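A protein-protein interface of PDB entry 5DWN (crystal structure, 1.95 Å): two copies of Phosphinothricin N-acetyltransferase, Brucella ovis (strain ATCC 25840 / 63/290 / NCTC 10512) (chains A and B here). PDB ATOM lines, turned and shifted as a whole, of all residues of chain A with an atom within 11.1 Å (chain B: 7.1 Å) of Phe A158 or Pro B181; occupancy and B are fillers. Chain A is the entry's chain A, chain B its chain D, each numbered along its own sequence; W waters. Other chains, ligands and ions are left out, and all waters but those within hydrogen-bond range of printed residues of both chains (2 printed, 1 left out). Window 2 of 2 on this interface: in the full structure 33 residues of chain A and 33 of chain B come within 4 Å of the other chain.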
ATOM      1  N   VAL A  31       6.883  16.173   6.602  1.00  0.00           N
ATOM      2  CA  VAL A  31       6.096  15.257   7.437  1.00  0.00           C
ATOM      3  C   VAL A  31       4.677  15.127   6.904  1.00  0.00           C
ATOM      4  O   VAL A  31       4.125  14.019   6.810  1.00  0.00           O
ATOM      5  CB  VAL A  31       6.098  15.731   8.903  1.00  0.00           C
ATOM      6  CG1 VAL A  31       5.064  14.953   9.715  1.00  0.00           C
ATOM      7  CG2 VAL A  31       7.491  15.568   9.523  1.00  0.00           C
ATOM      8  N   GLY A  34       4.974  13.834   2.758  1.00  0.00           N
ATOM      9  CA  GLY A  34       5.897  12.813   2.325  1.00  0.00           C
ATOM     10  C   GLY A  34       6.015  11.685   3.336  1.00  0.00           C
ATOM     11  O   GLY A  34       5.554  11.774   4.470  1.00  0.00           O
ATOM     12  N   THR A  35       6.662  10.616   2.885  1.00  0.00           N
ATOM     13  CA  THR A  35       6.881   9.405   3.663  1.00  0.00           C
ATOM     14  C   THR A  35       8.351   9.184   3.968  1.00  0.00           C
ATOM     15  O   THR A  35       8.717   8.116   4.468  1.00  0.00           O
ATOM     16  CB  THR A  35       6.331   8.203   2.903  1.00  0.00           C
ATOM     17  OG1 THR A  35       6.850   8.219   1.562  1.00  0.00           O
ATOM     18  CG2 THR A  35       4.798   8.246   2.862  1.00  0.00           C
ATOM     19  N   GLY A  36       9.210  10.147   3.644  1.00  0.00           N
ATOM     20  CA  GLY A  36      10.587  10.053   4.092  1.00  0.00           C
ATOM     21  C   GLY A  36      10.678  10.073   5.604  1.00  0.00           C
ATOM     22  O   GLY A  36      11.460   9.330   6.198  1.00  0.00           O
ATOM     23  N   SER A  37       9.854  10.898   6.245  1.00  0.00           N
ATOM     24  CA  SER A  37       9.759  10.913   7.694  1.00  0.00           C
ATOM     25  C   SER A  37       8.643   9.977   8.131  1.00  0.00           C
ATOM     26  O   SER A  37       7.563   9.957   7.529  1.00  0.00           O
ATOM     27  CB  SER A  37       9.490  12.327   8.225  1.00  0.00           C
ATOM     28  OG  SER A  37       9.144  12.308   9.628  1.00  0.00           O
ATOM     29  N   TYR A  38       8.906   9.200   9.177  1.00  0.00           N
ATOM     30  CA  TYR A  38       7.887   8.323   9.751  1.00  0.00           C
ATOM     31  C   TYR A  38       7.134   8.993  10.892  1.00  0.00           C
ATOM     32  O   TYR A  38       6.336   8.340  11.581  1.00  0.00           O
ATOM     33  CB  TYR A  38       8.505   7.002  10.221  1.00  0.00           C
ATOM     34  CG  TYR A  38       8.758   5.990   9.099  1.00  0.00           C
ATOM     35  CD1 TYR A  38       8.754   6.379   7.749  1.00  0.00           C
ATOM     36  CD2 TYR A  38       8.992   4.648   9.392  1.00  0.00           C
ATOM     37  CE1 TYR A  38       8.988   5.458   6.731  1.00  0.00           C
ATOM     38  CE2 TYR A  38       9.214   3.712   8.378  1.00  0.00           C
ATOM     39  CZ  TYR A  38       9.223   4.132   7.053  1.00  0.00           C
ATOM     40  OH  TYR A  38       9.457   3.208   6.063  1.00  0.00           O
ATOM     41  N   GLU A  39       7.371  10.275  11.112  1.00  0.00           N
ATOM     42  CA  GLU A  39       6.480  11.033  11.967  1.00  0.00           C
ATOM     43  C   GLU A  39       5.188  11.307  11.212  1.00  0.00           C
ATOM     44  O   GLU A  39       5.152  11.327   9.980  1.00  0.00           O
ATOM     45  CB  GLU A  39       7.144  12.335  12.408  1.00  0.00           C
ATOM     46  CG  GLU A  39       8.327  12.088  13.325  1.00  0.00           C
ATOM     47  CD  GLU A  39       8.749  13.327  14.078  1.00  0.00           C
ATOM     48  OE1 GLU A  39       9.601  14.068  13.561  1.00  0.00           O
ATOM     49  OE2 GLU A  39       8.230  13.545  15.188  1.00  0.00           O
ATOM     50  N   ILE A  40       4.111  11.457  11.965  1.00  0.00           N
ATOM     51  CA  ILE A  40       2.798  11.737  11.404  1.00  0.00           C
ATOM     52  C   ILE A  40       2.370  13.158  11.732  1.00  0.00           C
ATOM     53  O   ILE A  40       2.108  13.961  10.840  1.00  0.00           O
ATOM     54  CB  ILE A  40       1.754  10.710  11.895  1.00  0.00           C
ATOM     55  CG1 ILE A  40       2.277   9.282  11.728  1.00  0.00           C
ATOM     56  CG2 ILE A  40       0.428  10.918  11.174  1.00  0.00           C
ATOM     57  CD1 ILE A  40       2.133   8.720  10.363  1.00  0.00           C
ATOM     58  N   GLU A  41       2.287  13.478  12.988  1.00  0.00           N
ATOM     59  CA  GLU A  41       1.999  14.850  13.388  1.00  0.00           C
ATOM     60  C   GLU A  41       3.290  15.654  13.420  1.00  0.00           C
ATOM     61  O   GLU A  41       4.238  15.252  14.104  1.00  0.00           O
ATOM     62  CB  GLU A  41       1.334  14.881  14.760  1.00  0.00           C
ATOM     63  CG  GLU A  41       0.983  16.277  15.221  1.00  0.00           C
ATOM     64  CD  GLU A  41       0.172  16.259  16.494  1.00  0.00           C
ATOM     65  OE1 GLU A  41       0.220  15.231  17.204  1.00  0.00           O
ATOM     66  OE2 GLU A  41      -0.515  17.262  16.779  1.00  0.00           O
ATOM     67  N   GLY A 130      13.280   6.261   4.680  1.00  0.00           N
ATOM     68  CA  GLY A 130      11.893   5.846   4.800  1.00  0.00           C
ATOM     69  C   GLY A 130      11.243   5.704   3.431  1.00  0.00           C
ATOM     70  O   GLY A 130      11.502   6.487   2.518  1.00  0.00           O
ATOM     71  N   ASP A 131      10.391   4.681   3.290  1.00  0.00           N
ATOM     72  CA  ASP A 131       9.633   4.442   2.053  1.00  0.00           C
ATOM     73  C   ASP A 131      10.558   4.454   0.833  1.00  0.00           C
ATOM     74  O   ASP A 131      10.397   5.235  -0.107  1.00  0.00           O
ATOM     75  CB  ASP A 131       8.509   5.463   1.895  1.00  0.00           C
ATOM     76  CG  ASP A 131       7.548   5.121   0.755  1.00  0.00           C
ATOM     77  OD1 ASP A 131       7.598   3.986   0.232  1.00  0.00           O
ATOM     78  OD2 ASP A 131       6.716   5.984   0.402  1.00  0.00           O
ATOM     79  N   GLY A 132      11.560   3.579   0.879  1.00  0.00           N
ATOM     80  CA  GLY A 132      12.537   3.531  -0.199  1.00  0.00           C
ATOM     81  C   GLY A 132      11.939   3.202  -1.557  1.00  0.00           C
ATOM     82  O   GLY A 132      12.482   3.598  -2.592  1.00  0.00           O
ATOM     83  N   ILE A 153      14.268  -3.176   5.316  1.00  0.00           N
ATOM     84  CA  ILE A 153      13.287  -3.714   6.251  1.00  0.00           C
ATOM     85  C   ILE A 153      11.919  -3.551   5.595  1.00  0.00           C
ATOM     86  O   ILE A 153      11.432  -2.429   5.439  1.00  0.00           O
ATOM     87  CB  ILE A 153      13.347  -3.003   7.610  1.00  0.00           C
ATOM     88  CG1 ILE A 153      14.773  -3.017   8.173  1.00  0.00           C
ATOM     89  CG2 ILE A 153      12.384  -3.663   8.597  1.00  0.00           C
ATOM     90  CD1 ILE A 153      14.949  -2.116   9.406  1.00  0.00           C
ATOM     91  N   GLU A 154      11.305  -4.662   5.189  1.00  0.00           N
ATOM     92  CA  GLU A 154      10.031  -4.580   4.484  1.00  0.00           C
ATOM     93  C   GLU A 154       8.901  -4.297   5.454  1.00  0.00           C
ATOM     94  O   GLU A 154       8.880  -4.822   6.571  1.00  0.00           O
ATOM     95  CB  GLU A 154       9.730  -5.875   3.735  1.00  0.00           C
ATOM     96  CG  GLU A 154      10.520  -6.086   2.473  1.00  0.00           C
ATOM     97  CD  GLU A 154       9.999  -7.292   1.706  1.00  0.00           C
ATOM     98  OE1 GLU A 154       8.801  -7.298   1.338  1.00  0.00           O
ATOM     99  OE2 GLU A 154      10.778  -8.244   1.509  1.00  0.00           O
ATOM    100  N   GLY A 155       7.959  -3.464   5.022  1.00  0.00           N
ATOM    101  CA  GLY A 155       6.783  -3.171   5.836  1.00  0.00           C
ATOM    102  C   GLY A 155       7.101  -2.591   7.197  1.00  0.00           C
ATOM    103  O   GLY A 155       6.412  -2.900   8.182  1.00  0.00           O
ATOM    104  N   SER A 156       8.124  -1.738   7.273  1.00  0.00           N
ATOM    105  CA  SER A 156       8.555  -1.158   8.541  1.00  0.00           C
ATOM    106  C   SER A 156       7.661  -0.011   8.992  1.00  0.00           C
ATOM    107  O   SER A 156       7.601   0.274  10.192  1.00  0.00           O
ATOM    108  CB  SER A 156       9.986  -0.642   8.418  1.00  0.00           C
ATOM    109  OG  SER A 156      10.021   0.341   7.401  1.00  0.00           O
ATOM    110  N   GLY A 157       6.984   0.654   8.058  1.00  0.00           N
ATOM    111  CA  GLY A 157       6.136   1.778   8.388  1.00  0.00           C
ATOM    112  C   GLY A 157       4.786   1.660   7.708  1.00  0.00           C
ATOM    113  O   GLY A 157       4.638   1.006   6.680  1.00  0.00           O
ATOM    114  N   PHE A 158       3.791   2.302   8.311  1.00  0.00           N
ATOM    115  CA  PHE A 158       2.504   2.522   7.657  1.00  0.00           C
ATOM    116  C   PHE A 158       2.184   4.005   7.749  1.00  0.00           C
ATOM    117  O   PHE A 158       2.137   4.564   8.849  1.00  0.00           O
ATOM    118  CB  PHE A 158       1.390   1.688   8.290  1.00  0.00           C
ATOM    119  CG  PHE A 158       0.133   1.690   7.499  1.00  0.00           C
ATOM    120  CD1 PHE A 158      -0.019   0.837   6.408  1.00  0.00           C
ATOM    121  CD2 PHE A 158      -0.904   2.557   7.826  1.00  0.00           C
ATOM    122  CE1 PHE A 158      -1.195   0.848   5.658  1.00  0.00           C
ATOM    123  CE2 PHE A 158      -2.072   2.575   7.083  1.00  0.00           C
ATOM    124  CZ  PHE A 158      -2.218   1.716   5.995  1.00  0.00           C
ATOM    125  N   LYS A 159       1.968   4.641   6.601  1.00  0.00           N
ATOM    126  CA  LYS A 159       1.671   6.066   6.583  1.00  0.00           C
ATOM    127  C   LYS A 159       0.979   6.401   5.270  1.00  0.00           C
ATOM    128  O   LYS A 159       1.275   5.806   4.231  1.00  0.00           O
ATOM    129  CB  LYS A 159       2.952   6.897   6.752  1.00  0.00           C
ATOM    130  CG  LYS A 159       2.723   8.416   6.805  1.00  0.00           C
ATOM    131  CD  LYS A 159       4.033   9.158   7.130  1.00  0.00           C
ATOM    132  CE  LYS A 159       3.891  10.665   6.840  1.00  0.00           C
ATOM    133  NZ  LYS A 159       5.144  11.462   7.200  1.00  0.00           N
ATOM    134  N   HIS A 160       0.042   7.353   5.327  1.00  0.00           N
ATOM    135  CA  HIS A 160      -0.706   7.776   4.141  1.00  0.00           C
ATOM    136  C   HIS A 160      -1.397   6.598   3.458  1.00  0.00           C
ATOM    137  O   HIS A 160      -1.440   6.519   2.231  1.00  0.00           O
ATOM    138  CB  HIS A 160       0.192   8.499   3.136  1.00  0.00           C
ATOM    139  CG  HIS A 160       0.650   9.850   3.581  1.00  0.00           C
ATOM    140  ND1 HIS A 160       0.310  10.394   4.800  1.00  0.00           N
ATOM    141  CD2 HIS A 160       1.434  10.765   2.964  1.00  0.00           C
ATOM    142  CE1 HIS A 160       0.867  11.585   4.919  1.00  0.00           C
ATOM    143  NE2 HIS A 160       1.552  11.833   3.819  1.00  0.00           N
ATOM    144  N   GLY A 161      -1.929   5.674   4.253  1.00  0.00           N
ATOM    145  CA  GLY A 161      -2.663   4.533   3.736  1.00  0.00           C
ATOM    146  C   GLY A 161      -1.841   3.429   3.095  1.00  0.00           C
ATOM    147  O   GLY A 161      -2.431   2.530   2.492  1.00  0.00           O
ATOM    148  N   ARG A 162      -0.510   3.441   3.240  1.00  0.00           N
ATOM    149  CA  ARG A 162       0.402   2.567   2.508  1.00  0.00           C
ATOM    150  C   ARG A 162       1.410   1.924   3.451  1.00  0.00           C
ATOM    151  O   ARG A 162       1.932   2.592   4.342  1.00  0.00           O
ATOM    152  CB  ARG A 162       1.195   3.363   1.443  1.00  0.00           C
ATOM    153  CG  ARG A 162       0.507   3.465   0.108  1.00  0.00           C
ATOM    154  CD  ARG A 162       1.504   3.808  -0.985  1.00  0.00           C
ATOM    155  NE  ARG A 162       2.163   5.085  -0.755  1.00  0.00           N
ATOM    156  CZ  ARG A 162       3.457   5.224  -0.516  1.00  0.00           C
ATOM    157  NH1 ARG A 162       4.247   4.151  -0.483  1.00  0.00           N
ATOM    158  NH2 ARG A 162       3.958   6.440  -0.328  1.00  0.00           N
ATOM    159  N   TRP A 163       1.725   0.644   3.227  1.00  0.00           N
ATOM    160  CA  TRP A 163       2.888   0.047   3.874  1.00  0.00           C
ATOM    161  C   TRP A 163       4.160   0.564   3.222  1.00  0.00           C
ATOM    162  O   TRP A 163       4.205   0.773   2.008  1.00  0.00           O
ATOM    163  CB  TRP A 163       2.857  -1.477   3.778  1.00  0.00           C
ATOM    164  CG  TRP A 163       1.910  -2.103   4.742  1.00  0.00           C
ATOM    165  CD1 TRP A 163       0.740  -2.734   4.449  1.00  0.00           C
ATOM    166  CD2 TRP A 163       2.051  -2.148   6.169  1.00  0.00           C
ATOM    167  NE1 TRP A 163       0.136  -3.171   5.606  1.00  0.00           N
ATOM    168  CE2 TRP A 163       0.922  -2.823   6.676  1.00  0.00           C
ATOM    169  CE3 TRP A 163       3.022  -1.676   7.066  1.00  0.00           C
ATOM    170  CZ2 TRP A 163       0.739  -3.052   8.041  1.00  0.00           C
ATOM    171  CZ3 TRP A 163       2.837  -1.894   8.424  1.00  0.00           C
ATOM    172  CH2 TRP A 163       1.700  -2.579   8.897  1.00  0.00           C
ATOM    173  N   LEU A 164       5.207   0.738   4.034  1.00  0.00           N
ATOM    174  CA  LEU A 164       6.442   1.386   3.618  1.00  0.00           C
ATOM    175  C   LEU A 164       7.630   0.507   3.971  1.00  0.00           C
ATOM    176  O   LEU A 164       7.656  -0.105   5.042  1.00  0.00           O
ATOM    177  CB  LEU A 164       6.615   2.743   4.316  1.00  0.00           C
ATOM    178  CG  LEU A 164       5.391   3.654   4.387  1.00  0.00           C
ATOM    179  CD1 LEU A 164       5.721   4.886   5.241  1.00  0.00           C
ATOM    180  CD2 LEU A 164       4.955   4.056   2.992  1.00  0.00           C
ATOM    181  N   ASP A 165       8.627   0.484   3.093  1.00  0.00           N
ATOM    182  CA  ASP A 165       9.878  -0.219   3.361  1.00  0.00           C
ATOM    183  C   ASP A 165      10.976   0.773   3.715  1.00  0.00           C
ATOM    184  O   ASP A 165      11.070   1.850   3.120  1.00  0.00           O
ATOM    185  CB  ASP A 165      10.337  -1.028   2.148  1.00  0.00           C
ATOM    186  CG  ASP A 165       9.345  -2.088   1.732  1.00  0.00           C
ATOM    187  OD1 ASP A 165       8.482  -2.488   2.543  1.00  0.00           O
ATOM    188  OD2 ASP A 165       9.447  -2.513   0.577  1.00  0.00           O
ATOM    189  N   THR A 166      11.828   0.387   4.658  1.00  0.00           N
ATOM    190  CA  THR A 166      12.982   1.181   5.046  1.00  0.00           C
ATOM    191  C   THR A 166      14.201   0.673   4.292  1.00  0.00           C
ATOM    192  O   THR A 166      14.542  -0.509   4.390  1.00  0.00           O
ATOM    193  CB  THR A 166      13.230   1.077   6.544  1.00  0.00           C
ATOM    194  OG1 THR A 166      12.146   1.690   7.252  1.00  0.00           O
ATOM    195  CG2 THR A 166      14.551   1.772   6.890  1.00  0.00           C
ATOM    196  N   PRO B  84       5.686   7.382  14.939  1.00  0.00           N
ATOM    197  CA  PRO B  84       4.411   6.644  14.865  1.00  0.00           C
ATOM    198  C   PRO B  84       4.262   5.703  13.684  1.00  0.00           C
ATOM    199  O   PRO B  84       3.574   4.681  13.823  1.00  0.00           O
ATOM    200  CB  PRO B  84       3.368   7.772  14.812  1.00  0.00           C
ATOM    201  CG  PRO B  84       4.024   8.904  15.558  1.00  0.00           C
ATOM    202  CD  PRO B  84       5.474   8.825  15.158  1.00  0.00           C
ATOM    203  N   ALA B  85       4.861   5.989  12.525  1.00  0.00           N
ATOM    204  CA  ALA B  85       4.669   5.067  11.409  1.00  0.00           C
ATOM    205  C   ALA B  85       5.302   3.705  11.677  1.00  0.00           C
ATOM    206  O   ALA B  85       4.914   2.719  11.038  1.00  0.00           O
ATOM    207  CB  ALA B  85       5.221   5.647  10.104  1.00  0.00           C
ATOM    208  N   TYR B  86       6.238   3.624  12.620  1.00  0.00           N
ATOM    209  CA  TYR B  86       6.880   2.373  13.008  1.00  0.00           C
ATOM    210  C   TYR B  86       6.067   1.543  14.004  1.00  0.00           C
ATOM    211  O   TYR B  86       6.578   0.525  14.487  1.00  0.00           O
ATOM    212  CB  TYR B  86       8.231   2.654  13.665  1.00  0.00           C
ATOM    213  CG  TYR B  86       9.396   3.084  12.780  1.00  0.00           C
ATOM    214  CD1 TYR B  86       9.973   2.202  11.874  1.00  0.00           C
ATOM    215  CD2 TYR B  86       9.977   4.334  12.938  1.00  0.00           C
ATOM    216  CE1 TYR B  86      11.067   2.568  11.120  1.00  0.00           C
ATOM    217  CE2 TYR B  86      11.098   4.718  12.172  1.00  0.00           C
ATOM    218  CZ  TYR B  86      11.634   3.826  11.271  1.00  0.00           C
ATOM    219  OH  TYR B  86      12.743   4.176  10.503  1.00  0.00           O
ATOM    220  N   ARG B  87       4.833   1.920  14.343  1.00  0.00           N
ATOM    221  CA  ARG B  87       4.122   1.342  15.484  1.00  0.00           C
ATOM    222  C   ARG B  87       3.724  -0.118  15.296  1.00  0.00           C
ATOM    223  O   ARG B  87       3.285  -0.753  16.259  1.00  0.00           O
ATOM    224  CB  ARG B  87       2.868   2.168  15.787  1.00  0.00           C
ATOM    225  CG  ARG B  87       2.807   2.715  17.195  1.00  0.00           C
ATOM    226  CD  ARG B  87       3.293   4.151  17.269  1.00  0.00           C
ATOM    227  NE  ARG B  87       4.358   4.313  18.253  1.00  0.00           N
ATOM    228  CZ  ARG B  87       4.691   5.471  18.814  1.00  0.00           C
ATOM    229  NH1 ARG B  87       4.040   6.583  18.499  1.00  0.00           N
ATOM    230  NH2 ARG B  87       5.678   5.514  19.697  1.00  0.00           N
ATOM    231  N   TRP B  88       3.813  -0.657  14.086  1.00  0.00           N
ATOM    232  CA  TRP B  88       3.517  -2.068  13.853  1.00  0.00           C
ATOM    233  C   TRP B  88       4.789  -2.908  13.742  1.00  0.00           C
ATOM    234  O   TRP B  88       4.724  -4.092  13.389  1.00  0.00           O
ATOM    235  CB  TRP B  88       2.659  -2.239  12.594  1.00  0.00           C
ATOM    236  CG  TRP B  88       1.256  -1.672  12.726  1.00  0.00           C
ATOM    237  CD1 TRP B  88       0.127  -2.349  13.091  1.00  0.00           C
ATOM    238  CD2 TRP B  88       0.847  -0.315  12.487  1.00  0.00           C
ATOM    239  NE1 TRP B  88      -0.957  -1.503  13.092  1.00  0.00           N
ATOM    240  CE2 TRP B  88      -0.544  -0.250  12.720  1.00  0.00           C
ATOM    241  CE3 TRP B  88       1.520   0.841  12.077  1.00  0.00           C
ATOM    242  CZ2 TRP B  88      -1.278   0.935  12.578  1.00  0.00           C
ATOM    243  CZ3 TRP B  88       0.792   2.021  11.938  1.00  0.00           C
ATOM    244  CH2 TRP B  88      -0.592   2.057  12.186  1.00  0.00           C
ATOM    245  N   GLY B 121      -0.833  -7.669  17.853  1.00  0.00           N
ATOM    246  CA  GLY B 121      -1.169  -7.089  16.571  1.00  0.00           C
ATOM    247  C   GLY B 121      -0.022  -6.503  15.777  1.00  0.00           C
ATOM    248  O   GLY B 121      -0.278  -5.789  14.797  1.00  0.00           O
ATOM    249  N   ARG B 123       3.047  -6.369  13.046  1.00  0.00           N
ATOM    250  CA  ARG B 123       3.136  -6.913  11.694  1.00  0.00           C
ATOM    251  C   ARG B 123       4.533  -7.363  11.300  1.00  0.00           C
ATOM    252  O   ARG B 123       4.672  -8.125  10.337  1.00  0.00           O
ATOM    253  CB  ARG B 123       2.645  -5.877  10.668  1.00  0.00           C
ATOM    254  CG  ARG B 123       1.156  -5.547  10.776  1.00  0.00           C
ATOM    255  CD  ARG B 123       0.342  -6.822  10.714  1.00  0.00           C
ATOM    256  NE  ARG B 123      -1.100  -6.598  10.646  1.00  0.00           N
ATOM    257  CZ  ARG B 123      -1.768  -6.365   9.517  1.00  0.00           C
ATOM    258  NH1 ARG B 123      -1.118  -6.294   8.359  1.00  0.00           N
ATOM    259  NH2 ARG B 123      -3.085  -6.204   9.544  1.00  0.00           N
ATOM    260  N   GLY B 176       1.776  -9.415   7.766  1.00  0.00           N
ATOM    261  CA  GLY B 176       2.901  -8.585   7.364  1.00  0.00           C
ATOM    262  C   GLY B 176       2.414  -7.320   6.687  1.00  0.00           C
ATOM    263  O   GLY B 176       1.507  -6.640   7.177  1.00  0.00           O
ATOM    264  N   THR B 179      -1.530  -7.095   3.984  1.00  0.00           N
ATOM    265  CA  THR B 179      -2.902  -6.779   4.358  1.00  0.00           C
ATOM    266  C   THR B 179      -2.957  -5.418   5.035  1.00  0.00           C
ATOM    267  O   THR B 179      -1.970  -4.942   5.610  1.00  0.00           O
ATOM    268  CB  THR B 179      -3.477  -7.836   5.307  1.00  0.00           C
ATOM    269  OG1 THR B 179      -2.796  -7.753   6.563  1.00  0.00           O
ATOM    270  CG2 THR B 179      -3.259  -9.227   4.740  1.00  0.00           C
ATOM    271  N   GLU B 180      -4.129  -4.791   4.974  1.00  0.00           N
ATOM    272  CA  GLU B 180      -4.300  -3.508   5.645  1.00  0.00           C
ATOM    273  C   GLU B 180      -4.100  -3.679   7.151  1.00  0.00           C
ATOM    274  O   GLU B 180      -4.535  -4.685   7.728  1.00  0.00           O
ATOM    275  CB  GLU B 180      -5.686  -2.928   5.362  1.00  0.00           C
ATOM    276  N   PRO B 181      -3.448  -2.729   7.815  1.00  0.00           N
ATOM    277  CA  PRO B 181      -3.206  -2.857   9.256  1.00  0.00           C
ATOM    278  C   PRO B 181      -4.481  -2.678  10.057  1.00  0.00           C
ATOM    279  O   PRO B 181      -5.444  -2.043   9.624  1.00  0.00           O
ATOM    280  CB  PRO B 181      -2.229  -1.718   9.552  1.00  0.00           C
ATOM    281  CG  PRO B 181      -2.565  -0.696   8.528  1.00  0.00           C
ATOM    282  CD  PRO B 181      -2.902  -1.472   7.284  1.00  0.00           C
ATOM    283  N   GLY B 182      -4.467  -3.241  11.257  1.00  0.00           N
ATOM    284  CA  GLY B 182      -5.499  -2.958  12.219  1.00  0.00           C
ATOM    285  C   GLY B 182      -5.113  -1.744  13.031  1.00  0.00           C
ATOM    286  O   GLY B 182      -4.238  -0.959  12.643  1.00  0.00           O
ATOM    287  N   PRO B 183      -5.759  -1.561  14.175  1.00  0.00           N
ATOM    288  CA  PRO B 183      -5.336  -0.492  15.082  1.00  0.00           C
ATOM    289  C   PRO B 183      -3.895  -0.688  15.525  1.00  0.00           C
ATOM    290  O   PRO B 183      -3.365  -1.804  15.539  1.00  0.00           O
ATOM    291  CB  PRO B 183      -6.310  -0.614  16.261  1.00  0.00           C
ATOM    292  CG  PRO B 183      -6.913  -1.986  16.133  1.00  0.00           C
ATOM    293  CD  PRO B 183      -6.949  -2.272  14.668  1.00  0.00           C
ATOM    294  N   SER B 184      -3.258   0.423  15.859  1.00  0.00           N
ATOM    295  CA  SER B 184      -1.889   0.395  16.343  1.00  0.00           C
ATOM    296  C   SER B 184      -1.791  -0.490  17.584  1.00  0.00           C
ATOM    297  O   SER B 184      -2.582  -0.319  18.521  1.00  0.00           O
ATOM    298  CB  SER B 184      -1.445   1.820  16.665  1.00  0.00           C
ATOM    299  OG  SER B 184      -0.569   1.873  17.780  1.00  0.00           O
HETATM  300  O   HOH W   1      12.612   4.234   7.903  1.00  0.00           O
HETATM  301  O   HOH W   2       5.937  -2.912  10.930  1.00  0.00           O
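Water W1 lies within hydrogen-bond range of the side-chain hydroxyl of Tyr B86 (2.6 Å) and the side-chain hydroxyl of Thr A166 (2.7 Å). Water W2 bridges the backbone carbonyl oxygen of Gly A155 (2.8 Å) and the backbone carbonyl oxygen of Trp B88 (3.0 Å).
No position is printed for both chains. Of the 15 pairs that touch across the chains among the printed residues, none has its exchanged pair printed and touching as well.
NE1 of Trp A163 lies within hydrogen-bond range of O of Thr B179, at 2.8 Å. The backbone carbonyl oxygen of Ala B85 sits at hydrogen-bond distance from the backbone NH of Phe A158 (3.0 Å). The backbone carbonyl oxygen (O) of Tyr A38 lies within hydrogen-bond range of the backbone NH (N) of Ala B85 (2.9 Å).
Hydrophobic or aromatic side chains of chain A that line the printed part of chain B: Tyr A38, Ile A40, Phe A158 and Trp A163. Among the printed residues, 15 pairs touch across the chains.
Phe A158 touches just these residues of chain B: Ala B85, Trp B88 and Pro B181. Pro B181 touches two residues of chain A. Ala B85 touches four residues of chain A. No residue of chain A comes within 4 Å of Glu B180. No residue of chain A comes within 4 Å of Gly B182. No residue of chain A comes within 4 Å of Pro B183. Of the printed residues of chain A, Gly B176 touches Trp A163. Of the printed residues of chain A, Pro B84 touches Tyr A38 (3.6 Å) and Ile A40 (3.6 Å). Printed residues of chain B within 4 Å of Ser A156: Ala B85 (3.7 Å) and Tyr B86 (3.5 Å). Of the printed residues of chain A, Tyr B86 touches Tyr A38 (3.3 Å) and Ser A156 (3.5 Å). Thr A166 touches none of the printed residues of chain B.
OH of Tyr A38 sits at hydrogen-bond distance from OG of Ser A156 (3.2 Å). The guanidinium group of Arg B123 lies within hydrogen-bond range of the backbone carbonyl oxygen of Glu B180. NE1 of Trp B88 lies within hydrogen-bond range of O of Gly B182 (3.4 Å). The indole nitrogen of Trp B88 lies within hydrogen-bond range of the backbone carbonyl oxygen of Pro B183. The backbone NH (N) of Leu A164 sits at hydrogen-bond distance from the backbone carbonyl oxygen (O) of Gly A157 (2.7 Å). NH1 of Arg B123 is in hydrogen-bond range of O of Gly B176 (2.9 Å).
O of Tyr A38 touches N of Pro B84, at 3.6 Å. Tyr A38 touches Tyr B86 (CD2 to CZ, 3.3 Å). Pro B84 touches Ile A40 (CB to CG1, 3.6 Å). O of Ser A156 touches CD1 of Tyr B86, 3.5 Å away. Trp B88 touches Phe A158. Phe A158 touches Pro B181. CH2 of Trp A163 touches CB of Trp B88, 3.8 Å away. CH2 of Trp A163 touches CG of Arg B123, at 3.6 Å. Trp A163 touches Gly B176. Trp A163 touches Pro B181 (CZ2 to CB, 3.6 Å).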
